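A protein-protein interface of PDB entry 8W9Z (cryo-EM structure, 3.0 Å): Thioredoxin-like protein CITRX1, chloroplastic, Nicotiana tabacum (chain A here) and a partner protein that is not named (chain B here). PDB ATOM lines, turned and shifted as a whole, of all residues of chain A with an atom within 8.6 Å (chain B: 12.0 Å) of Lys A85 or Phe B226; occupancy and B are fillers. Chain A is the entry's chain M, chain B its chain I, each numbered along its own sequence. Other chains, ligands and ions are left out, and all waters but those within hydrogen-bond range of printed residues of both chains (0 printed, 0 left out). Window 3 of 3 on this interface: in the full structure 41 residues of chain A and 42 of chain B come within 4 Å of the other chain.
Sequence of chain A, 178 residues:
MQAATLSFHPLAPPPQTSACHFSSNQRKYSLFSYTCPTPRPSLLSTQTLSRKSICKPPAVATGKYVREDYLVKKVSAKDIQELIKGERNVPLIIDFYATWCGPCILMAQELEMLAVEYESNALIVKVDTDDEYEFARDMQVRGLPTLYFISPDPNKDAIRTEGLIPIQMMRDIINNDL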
ATOM      1  N   ALA A  77     -14.569 -13.301  18.487  1.00  0.00           N
ATOM      2  CA  ALA A  77     -14.559 -11.857  18.686  1.00  0.00           C
ATOM      3  C   ALA A  77     -15.960 -11.261  18.672  1.00  0.00           C
ATOM      4  O   ALA A  77     -16.164 -10.184  19.239  1.00  0.00           O
ATOM      5  CB  ALA A  77     -13.696 -11.183  17.619  1.00  0.00           C
ATOM      6  N   LYS A  78     -16.923 -11.932  18.040  1.00  0.00           N
ATOM      7  CA  LYS A  78     -18.293 -11.433  18.032  1.00  0.00           C
ATOM      8  C   LYS A  78     -19.041 -11.802  19.305  1.00  0.00           C
ATOM      9  O   LYS A  78     -19.889 -11.030  19.766  1.00  0.00           O
ATOM     10  CB  LYS A  78     -19.041 -11.967  16.810  1.00  0.00           C
ATOM     11  CG  LYS A  78     -18.429 -11.558  15.480  1.00  0.00           C
ATOM     12  CD  LYS A  78     -19.220 -12.122  14.311  1.00  0.00           C
ATOM     13  CE  LYS A  78     -18.612 -11.708  12.981  1.00  0.00           C
ATOM     14  NZ  LYS A  78     -17.210 -12.188  12.838  1.00  0.00           N
ATOM     15  N   ASP A  79     -18.739 -12.965  19.888  1.00  0.00           N
ATOM     16  CA  ASP A  79     -19.394 -13.360  21.130  1.00  0.00           C
ATOM     17  C   ASP A  79     -19.032 -12.415  22.268  1.00  0.00           C
ATOM     18  O   ASP A  79     -19.881 -12.083  23.104  1.00  0.00           O
ATOM     19  CB  ASP A  79     -19.020 -14.799  21.485  1.00  0.00           C
ATOM     20  CG  ASP A  79     -19.427 -15.788  20.412  1.00  0.00           C
ATOM     21  OD1 ASP A  79     -20.428 -15.527  19.712  1.00  0.00           O
ATOM     22  OD2 ASP A  79     -18.747 -16.824  20.267  1.00  0.00           O
ATOM     23  N   ILE A  80     -17.777 -11.965  22.315  1.00  0.00           N
ATOM     24  CA  ILE A  80     -17.362 -11.020  23.349  1.00  0.00           C
ATOM     25  C   ILE A  80     -18.123  -9.707  23.203  1.00  0.00           C
ATOM     26  O   ILE A  80     -18.619  -9.142  24.186  1.00  0.00           O
ATOM     27  CB  ILE A  80     -15.839 -10.801  23.294  1.00  0.00           C
ATOM     28  CG1 ILE A  80     -15.103 -12.068  23.731  1.00  0.00           C
ATOM     29  CG2 ILE A  80     -15.435  -9.623  24.166  1.00  0.00           C
ATOM     30  CD1 ILE A  80     -15.362 -12.452  25.170  1.00  0.00           C
ATOM     31  N   GLN A  81     -18.233  -9.208  21.970  1.00  0.00           N
ATOM     32  CA  GLN A  81     -18.951  -7.959  21.741  1.00  0.00           C
ATOM     33  C   GLN A  81     -20.434  -8.106  22.057  1.00  0.00           C
ATOM     34  O   GLN A  81     -21.069  -7.156  22.530  1.00  0.00           O
ATOM     35  CB  GLN A  81     -18.748  -7.496  20.299  1.00  0.00           C
ATOM     36  CG  GLN A  81     -17.303  -7.175  19.956  1.00  0.00           C
ATOM     37  CD  GLN A  81     -17.129  -6.726  18.520  1.00  0.00           C
ATOM     38  OE1 GLN A  81     -18.085  -6.700  17.746  1.00  0.00           O
ATOM     39  NE2 GLN A  81     -15.903  -6.370  18.157  1.00  0.00           N
ATOM     40  N   GLU A  82     -21.005  -9.286  21.807  1.00  0.00           N
ATOM     41  CA  GLU A  82     -22.406  -9.508  22.151  1.00  0.00           C
ATOM     42  C   GLU A  82     -22.603  -9.617  23.657  1.00  0.00           C
ATOM     43  O   GLU A  82     -23.656  -9.223  24.172  1.00  0.00           O
ATOM     44  CB  GLU A  82     -22.929 -10.762  21.454  1.00  0.00           C
ATOM     45  CG  GLU A  82     -23.072 -10.622  19.948  1.00  0.00           C
ATOM     46  CD  GLU A  82     -23.612 -11.877  19.293  1.00  0.00           C
ATOM     47  OE1 GLU A  82     -23.905 -12.850  20.019  1.00  0.00           O
ATOM     48  OE2 GLU A  82     -23.744 -11.890  18.051  1.00  0.00           O
ATOM     49  N   LEU A  83     -21.613 -10.147  24.378  1.00  0.00           N
ATOM     50  CA  LEU A  83     -21.706 -10.235  25.829  1.00  0.00           C
ATOM     51  C   LEU A  83     -21.435  -8.905  26.516  1.00  0.00           C
ATOM     52  O   LEU A  83     -21.889  -8.706  27.648  1.00  0.00           O
ATOM     53  CB  LEU A  83     -20.733 -11.287  26.363  1.00  0.00           C
ATOM     54  CG  LEU A  83     -21.047 -12.751  26.052  1.00  0.00           C
ATOM     55  CD1 LEU A  83     -19.986 -13.662  26.647  1.00  0.00           C
ATOM     56  CD2 LEU A  83     -22.428 -13.126  26.564  1.00  0.00           C
ATOM     57  N   ILE A  84     -20.711  -7.998  25.869  1.00  0.00           N
ATOM     58  CA  ILE A  84     -20.432  -6.695  26.467  1.00  0.00           C
ATOM     59  C   ILE A  84     -21.573  -5.715  26.230  1.00  0.00           C
ATOM     60  O   ILE A  84     -21.957  -4.970  27.136  1.00  0.00           O
ATOM     61  CB  ILE A  84     -19.095  -6.145  25.934  1.00  0.00           C
ATOM     62  CG1 ILE A  84     -17.937  -7.006  26.432  1.00  0.00           C
ATOM     63  CG2 ILE A  84     -18.898  -4.701  26.361  1.00  0.00           C
ATOM     64  CD1 ILE A  84     -17.957  -7.227  27.923  1.00  0.00           C
ATOM     65  N   LYS A  85     -22.145  -5.705  25.023  1.00  0.00           N
ATOM     66  CA  LYS A  85     -23.221  -4.772  24.714  1.00  0.00           C
ATOM     67  C   LYS A  85     -24.521  -5.106  25.433  1.00  0.00           C
ATOM     68  O   LYS A  85     -25.439  -4.279  25.426  1.00  0.00           O
ATOM     69  CB  LYS A  85     -23.470  -4.735  23.206  1.00  0.00           C
ATOM     70  CG  LYS A  85     -24.091  -6.005  22.647  1.00  0.00           C
ATOM     71  CD  LYS A  85     -24.388  -5.866  21.162  1.00  0.00           C
ATOM     72  CE  LYS A  85     -23.119  -5.603  20.369  1.00  0.00           C
ATOM     73  NZ  LYS A  85     -23.398  -5.423  18.918  1.00  0.00           N
ATOM     74  N   GLY A  86     -24.625  -6.285  26.047  1.00  0.00           N
ATOM     75  CA  GLY A  86     -25.821  -6.690  26.749  1.00  0.00           C
ATOM     76  C   GLY A  86     -25.737  -6.423  28.242  1.00  0.00           C
ATOM     77  O   GLY A  86     -24.870  -5.701  28.734  1.00  0.00           O
ATOM     78  N   GLU A  87     -26.670  -7.030  28.969  1.00  0.00           N
ATOM     79  CA  GLU A  87     -26.746  -6.903  30.415  1.00  0.00           C
ATOM     80  C   GLU A  87     -26.327  -8.210  31.075  1.00  0.00           C
ATOM     81  O   GLU A  87     -26.484  -9.293  30.504  1.00  0.00           O
ATOM     82  CB  GLU A  87     -28.159  -6.517  30.869  1.00  0.00           C
ATOM     83  CG  GLU A  87     -29.254  -7.489  30.448  1.00  0.00           C
ATOM     84  CD  GLU A  87     -29.729  -7.262  29.025  1.00  0.00           C
ATOM     85  OE1 GLU A  87     -29.269  -6.290  28.390  1.00  0.00           O
ATOM     86  OE2 GLU A  87     -30.563  -8.055  28.542  1.00  0.00           O
ATOM     87  N   ARG A  88     -25.789  -8.097  32.286  1.00  0.00           N
ATOM     88  CA  ARG A  88     -25.272  -9.252  33.003  1.00  0.00           C
ATOM     89  C   ARG A  88     -25.293  -8.964  34.496  1.00  0.00           C
ATOM     90  O   ARG A  88     -25.283  -7.808  34.926  1.00  0.00           O
ATOM     91  CB  ARG A  88     -23.852  -9.598  32.542  1.00  0.00           C
ATOM     92  CG  ARG A  88     -22.868  -8.458  32.726  1.00  0.00           C
ATOM     93  CD  ARG A  88     -21.667  -8.597  31.810  1.00  0.00           C
ATOM     94  NE  ARG A  88     -20.770  -7.453  31.934  1.00  0.00           N
ATOM     95  CZ  ARG A  88     -20.923  -6.311  31.273  1.00  0.00           C
ATOM     96  NH1 ARG A  88     -21.940  -6.158  30.437  1.00  0.00           N
ATOM     97  NH2 ARG A  88     -20.060  -5.320  31.446  1.00  0.00           N
ATOM     98  N   LEU A  92     -17.242 -10.918  34.339  1.00  0.00           N
ATOM     99  CA  LEU A  92     -16.742 -11.561  33.131  1.00  0.00           C
ATOM    100  C   LEU A  92     -15.223 -11.482  33.118  1.00  0.00           C
ATOM    101  O   LEU A  92     -14.652 -10.422  33.394  1.00  0.00           O
ATOM    102  CB  LEU A  92     -17.320 -10.902  31.877  1.00  0.00           C
ATOM    103  CG  LEU A  92     -16.803 -11.411  30.532  1.00  0.00           C
ATOM    104  CD1 LEU A  92     -17.125 -12.884  30.353  1.00  0.00           C
ATOM    105  CD2 LEU A  92     -17.380 -10.591  29.393  1.00  0.00           C
ATOM    106  N   PHE A 135      -8.788  -8.246  16.838  1.00  0.00           N
ATOM    107  CA  PHE A 135      -9.549  -7.910  18.035  1.00  0.00           C
ATOM    108  C   PHE A 135      -8.646  -7.788  19.254  1.00  0.00           C
ATOM    109  O   PHE A 135      -8.902  -6.957  20.132  1.00  0.00           O
ATOM    110  CB  PHE A 135     -10.636  -8.955  18.282  1.00  0.00           C
ATOM    111  CG  PHE A 135     -11.464  -8.688  19.506  1.00  0.00           C
ATOM    112  CD1 PHE A 135     -12.486  -7.756  19.477  1.00  0.00           C
ATOM    113  CD2 PHE A 135     -11.225  -9.374  20.683  1.00  0.00           C
ATOM    114  CE1 PHE A 135     -13.250  -7.510  20.600  1.00  0.00           C
ATOM    115  CE2 PHE A 135     -11.985  -9.132  21.809  1.00  0.00           C
ATOM    116  CZ  PHE A 135     -12.998  -8.200  21.767  1.00  0.00           C
ATOM    117  N   MET A 139      -8.040  -4.220  21.531  1.00  0.00           N
ATOM    118  CA  MET A 139      -8.179  -4.157  22.981  1.00  0.00           C
ATOM    119  C   MET A 139      -6.930  -3.624  23.675  1.00  0.00           C
ATOM    120  O   MET A 139      -6.842  -3.717  24.904  1.00  0.00           O
ATOM    121  CB  MET A 139      -8.524  -5.542  23.535  1.00  0.00           C
ATOM    122  CG  MET A 139      -9.888  -6.062  23.115  1.00  0.00           C
ATOM    123  SD  MET A 139     -11.238  -5.330  24.054  1.00  0.00           S
ATOM    124  CE  MET A 139     -10.893  -5.961  25.694  1.00  0.00           C
ATOM    125  N   PRO A 154     -22.400  -1.280  34.304  1.00  0.00           N
ATOM    126  CA  PRO A 154     -21.819  -0.638  33.129  1.00  0.00           C
ATOM    127  C   PRO A 154     -21.447   0.800  33.386  1.00  0.00           C
ATOM    128  O   PRO A 154     -21.818   1.674  32.619  1.00  0.00           O
ATOM    129  CB  PRO A 154     -22.918  -0.744  32.098  1.00  0.00           C
ATOM    130  CG  PRO A 154     -24.182  -0.775  32.886  1.00  0.00           C
ATOM    131  CD  PRO A 154     -23.861  -1.422  34.199  1.00  0.00           C
ATOM    132  N   MET B 222      -9.426   0.496  32.261  1.00  0.00           N
ATOM    133  CA  MET B 222      -9.797   0.848  30.900  1.00  0.00           C
ATOM    134  C   MET B 222     -11.312   0.945  30.793  1.00  0.00           C
ATOM    135  O   MET B 222     -12.052   0.317  31.553  1.00  0.00           O
ATOM    136  CB  MET B 222      -9.269  -0.172  29.882  1.00  0.00           C
ATOM    137  CG  MET B 222      -7.762  -0.159  29.707  1.00  0.00           C
ATOM    138  SD  MET B 222      -7.228  -1.234  28.363  1.00  0.00           S
ATOM    139  CE  MET B 222      -5.471  -0.896  28.337  1.00  0.00           C
ATOM    140  N   LYS B 223     -11.764   1.743  29.830  1.00  0.00           N
ATOM    141  CA  LYS B 223     -13.180   1.927  29.549  1.00  0.00           C
ATOM    142  C   LYS B 223     -13.503   1.294  28.202  1.00  0.00           C
ATOM    143  O   LYS B 223     -12.795   1.530  27.217  1.00  0.00           O
ATOM    144  CB  LYS B 223     -13.550   3.411  29.547  1.00  0.00           C
ATOM    145  CG  LYS B 223     -15.043   3.680  29.596  1.00  0.00           C
ATOM    146  CD  LYS B 223     -15.333   5.171  29.683  1.00  0.00           C
ATOM    147  CE  LYS B 223     -14.706   5.784  30.924  1.00  0.00           C
ATOM    148  NZ  LYS B 223     -14.967   7.248  31.013  1.00  0.00           N
ATOM    149  N   ILE B 224     -14.567   0.490  28.165  1.00  0.00           N
ATOM    150  CA  ILE B 224     -14.889  -0.272  26.961  1.00  0.00           C
ATOM    151  C   ILE B 224     -15.324   0.659  25.833  1.00  0.00           C
ATOM    152  O   ILE B 224     -14.694   0.705  24.770  1.00  0.00           O
ATOM    153  CB  ILE B 224     -15.958  -1.335  27.266  1.00  0.00           C
ATOM    154  CG1 ILE B 224     -16.985  -0.799  28.268  1.00  0.00           C
ATOM    155  CG2 ILE B 224     -15.306  -2.602  27.796  1.00  0.00           C
ATOM    156  CD1 ILE B 224     -18.082  -1.785  28.606  1.00  0.00           C
ATOM    157  N   LYS B 225     -16.405   1.412  26.049  1.00  0.00           N
ATOM    158  CA  LYS B 225     -16.921   2.379  25.079  1.00  0.00           C
ATOM    159  C   LYS B 225     -17.204   1.717  23.727  1.00  0.00           C
ATOM    160  O   LYS B 225     -16.564   2.006  22.713  1.00  0.00           O
ATOM    161  CB  LYS B 225     -15.963   3.565  24.918  1.00  0.00           C
ATOM    162  CG  LYS B 225     -15.850   4.447  26.148  1.00  0.00           C
ATOM    163  CD  LYS B 225     -14.996   5.673  25.869  1.00  0.00           C
ATOM    164  CE  LYS B 225     -13.593   5.284  25.428  1.00  0.00           C
ATOM    165  NZ  LYS B 225     -12.757   6.478  25.128  1.00  0.00           N
ATOM    166  N   PHE B 226     -18.181   0.812  23.731  1.00  0.00           N
ATOM    167  CA  PHE B 226     -18.588   0.135  22.505  1.00  0.00           C
ATOM    168  C   PHE B 226     -19.436   1.061  21.641  1.00  0.00           C
ATOM    169  O   PHE B 226     -20.660   1.116  21.796  1.00  0.00           O
ATOM    170  CB  PHE B 226     -19.354  -1.148  22.828  1.00  0.00           C
ATOM    171  CG  PHE B 226     -19.649  -1.997  21.624  1.00  0.00           C
ATOM    172  CD1 PHE B 226     -18.699  -2.875  21.131  1.00  0.00           C
ATOM    173  CD2 PHE B 226     -20.878  -1.921  20.989  1.00  0.00           C
ATOM    174  CE1 PHE B 226     -18.966  -3.659  20.023  1.00  0.00           C
ATOM    175  CE2 PHE B 226     -21.151  -2.700  19.881  1.00  0.00           C
ATOM    176  CZ  PHE B 226     -20.194  -3.570  19.398  1.00  0.00           C
ATOM    177  N   GLU B 227     -18.794   1.792  20.729  1.00  0.00           N
ATOM    178  CA  GLU B 227     -19.471   2.738  19.841  1.00  0.00           C
ATOM    179  C   GLU B 227     -19.035   2.433  18.410  1.00  0.00           C
ATOM    180  O   GLU B 227     -18.004   2.933  17.951  1.00  0.00           O
ATOM    181  CB  GLU B 227     -19.157   4.180  20.232  1.00  0.00           C
ATOM    182  N   ASP B 228     -19.821   1.608  17.716  1.00  0.00           N
ATOM    183  CA  ASP B 228     -19.551   1.190  16.341  1.00  0.00           C
ATOM    184  C   ASP B 228     -18.200   0.495  16.202  1.00  0.00           C
ATOM    185  O   ASP B 228     -17.634   0.444  15.105  1.00  0.00           O
ATOM    186  CB  ASP B 228     -19.640   2.374  15.370  1.00  0.00           C
ATOM    187  N   GLY B 229     -17.674  -0.039  17.300  1.00  0.00           N
ATOM    188  CA  GLY B 229     -16.381  -0.694  17.293  1.00  0.00           C
ATOM    189  C   GLY B 229     -15.768  -0.746  18.676  1.00  0.00           C
ATOM    190  O   GLY B 229     -15.966   0.168  19.482  1.00  0.00           O
ATOM    191  N   LYS B 230     -15.022  -1.806  18.965  1.00  0.00           N
ATOM    192  CA  LYS B 230     -14.390  -1.972  20.271  1.00  0.00           C
ATOM    193  C   LYS B 230     -13.172  -1.061  20.337  1.00  0.00           C
ATOM    194  O   LYS B 230     -12.110  -1.381  19.799  1.00  0.00           O
ATOM    195  CB  LYS B 230     -14.010  -3.430  20.500  1.00  0.00           C
ATOM    196  CG  LYS B 230     -13.553  -3.734  21.914  1.00  0.00           C
ATOM    197  CD  LYS B 230     -14.683  -3.540  22.913  1.00  0.00           C
ATOM    198  CE  LYS B 230     -15.826  -4.502  22.642  1.00  0.00           C
ATOM    199  NZ  LYS B 230     -16.945  -4.319  23.605  1.00  0.00           N
ATOM    200  N   MET B 231     -13.322   0.084  21.000  1.00  0.00           N
ATOM    201  CA  MET B 231     -12.250   1.071  21.134  1.00  0.00           C
ATOM    202  C   MET B 231     -12.103   1.419  22.613  1.00  0.00           C
ATOM    203  O   MET B 231     -12.925   2.155  23.167  1.00  0.00           O
ATOM    204  CB  MET B 231     -12.540   2.314  20.297  1.00  0.00           C
ATOM    205  N   LYS B 232     -11.053   0.899  23.242  1.00  0.00           N
ATOM    206  CA  LYS B 232     -10.800   1.109  24.659  1.00  0.00           C
ATOM    207  C   LYS B 232      -9.788   2.230  24.863  1.00  0.00           C
ATOM    208  O   LYS B 232      -8.923   2.473  24.018  1.00  0.00           O
ATOM    209  CB  LYS B 232     -10.295  -0.177  25.315  1.00  0.00           C
ATOM    210  N   VAL B 233      -9.908   2.914  26.000  1.00  0.00           N
ATOM    211  CA  VAL B 233      -9.022   4.013  26.362  1.00  0.00           C
ATOM    212  C   VAL B 233      -8.518   3.787  27.781  1.00  0.00           C
ATOM    213  O   VAL B 233      -9.235   3.239  28.625  1.00  0.00           O
ATOM    214  CB  VAL B 233      -9.731   5.378  26.249  1.00  0.00           C
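Among the printed residues, merely in contact across the chains: Gln A81 with Phe B226 (3.9 Å), Ile A84 with Ile B224 (3.8 Å), Ile A84 with Lys B230 (3.4 Å), Lys A85 with Phe B226 (3.5 Å) and Met A139 with Lys B230 (3.5 Å).
Lys A85 touches just one residue of chain B: Phe B226. Of the printed residues of chain A, Phe B226 touches Gln A81 (3.9 Å) and Lys A85 (3.5 Å). Of chain B, only Phe B226 comes within 4 Å of Gln A81. No residue of chain B comes within 4 Å of Glu A82. Gly A86 touches none of the printed residues of chain B. Glu A87 touches none of the printed residues of chain B. No residue of chain A comes within 4 Å of Glu B227. Printed residues of chain A within 4 Å of Ile B224: Ile A84 (3.8 Å). Printed residues of chain A within 4 Å of Lys B230: Ile A84 (3.4 Å) and Met A139 (3.5 Å). Printed residues of chain B within 4 Å of Met A139: Lys B230. Ala A77 touches none of the printed residues of chain B. Asp B228 touches none of the printed residues of chain A. The nearest residue of chain A that does not touch Phe B226 is Ile A84 (5.0 Å).
Printed residues of chain B that touch a printed residue of chain A: Ile B224, Phe B226 and Lys B230. Hydrophobic or aromatic side chains of chain B that line the printed part of chain A: Ile B224 and Phe B226. Along chain B the printed residues that touch a printed residue of chain A span positions 224 to 230. Hydrophobic or aromatic side chains of chain A within 4 Å of the printed part of chain B: Ile A84 and Met A139. Among the printed residues, 5 pairs touch across the chains. Among the printed residues, no Asp or Glu carboxylate lies within 4 Å of a Lys or Arg side-chain nitrogen of the other chain.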
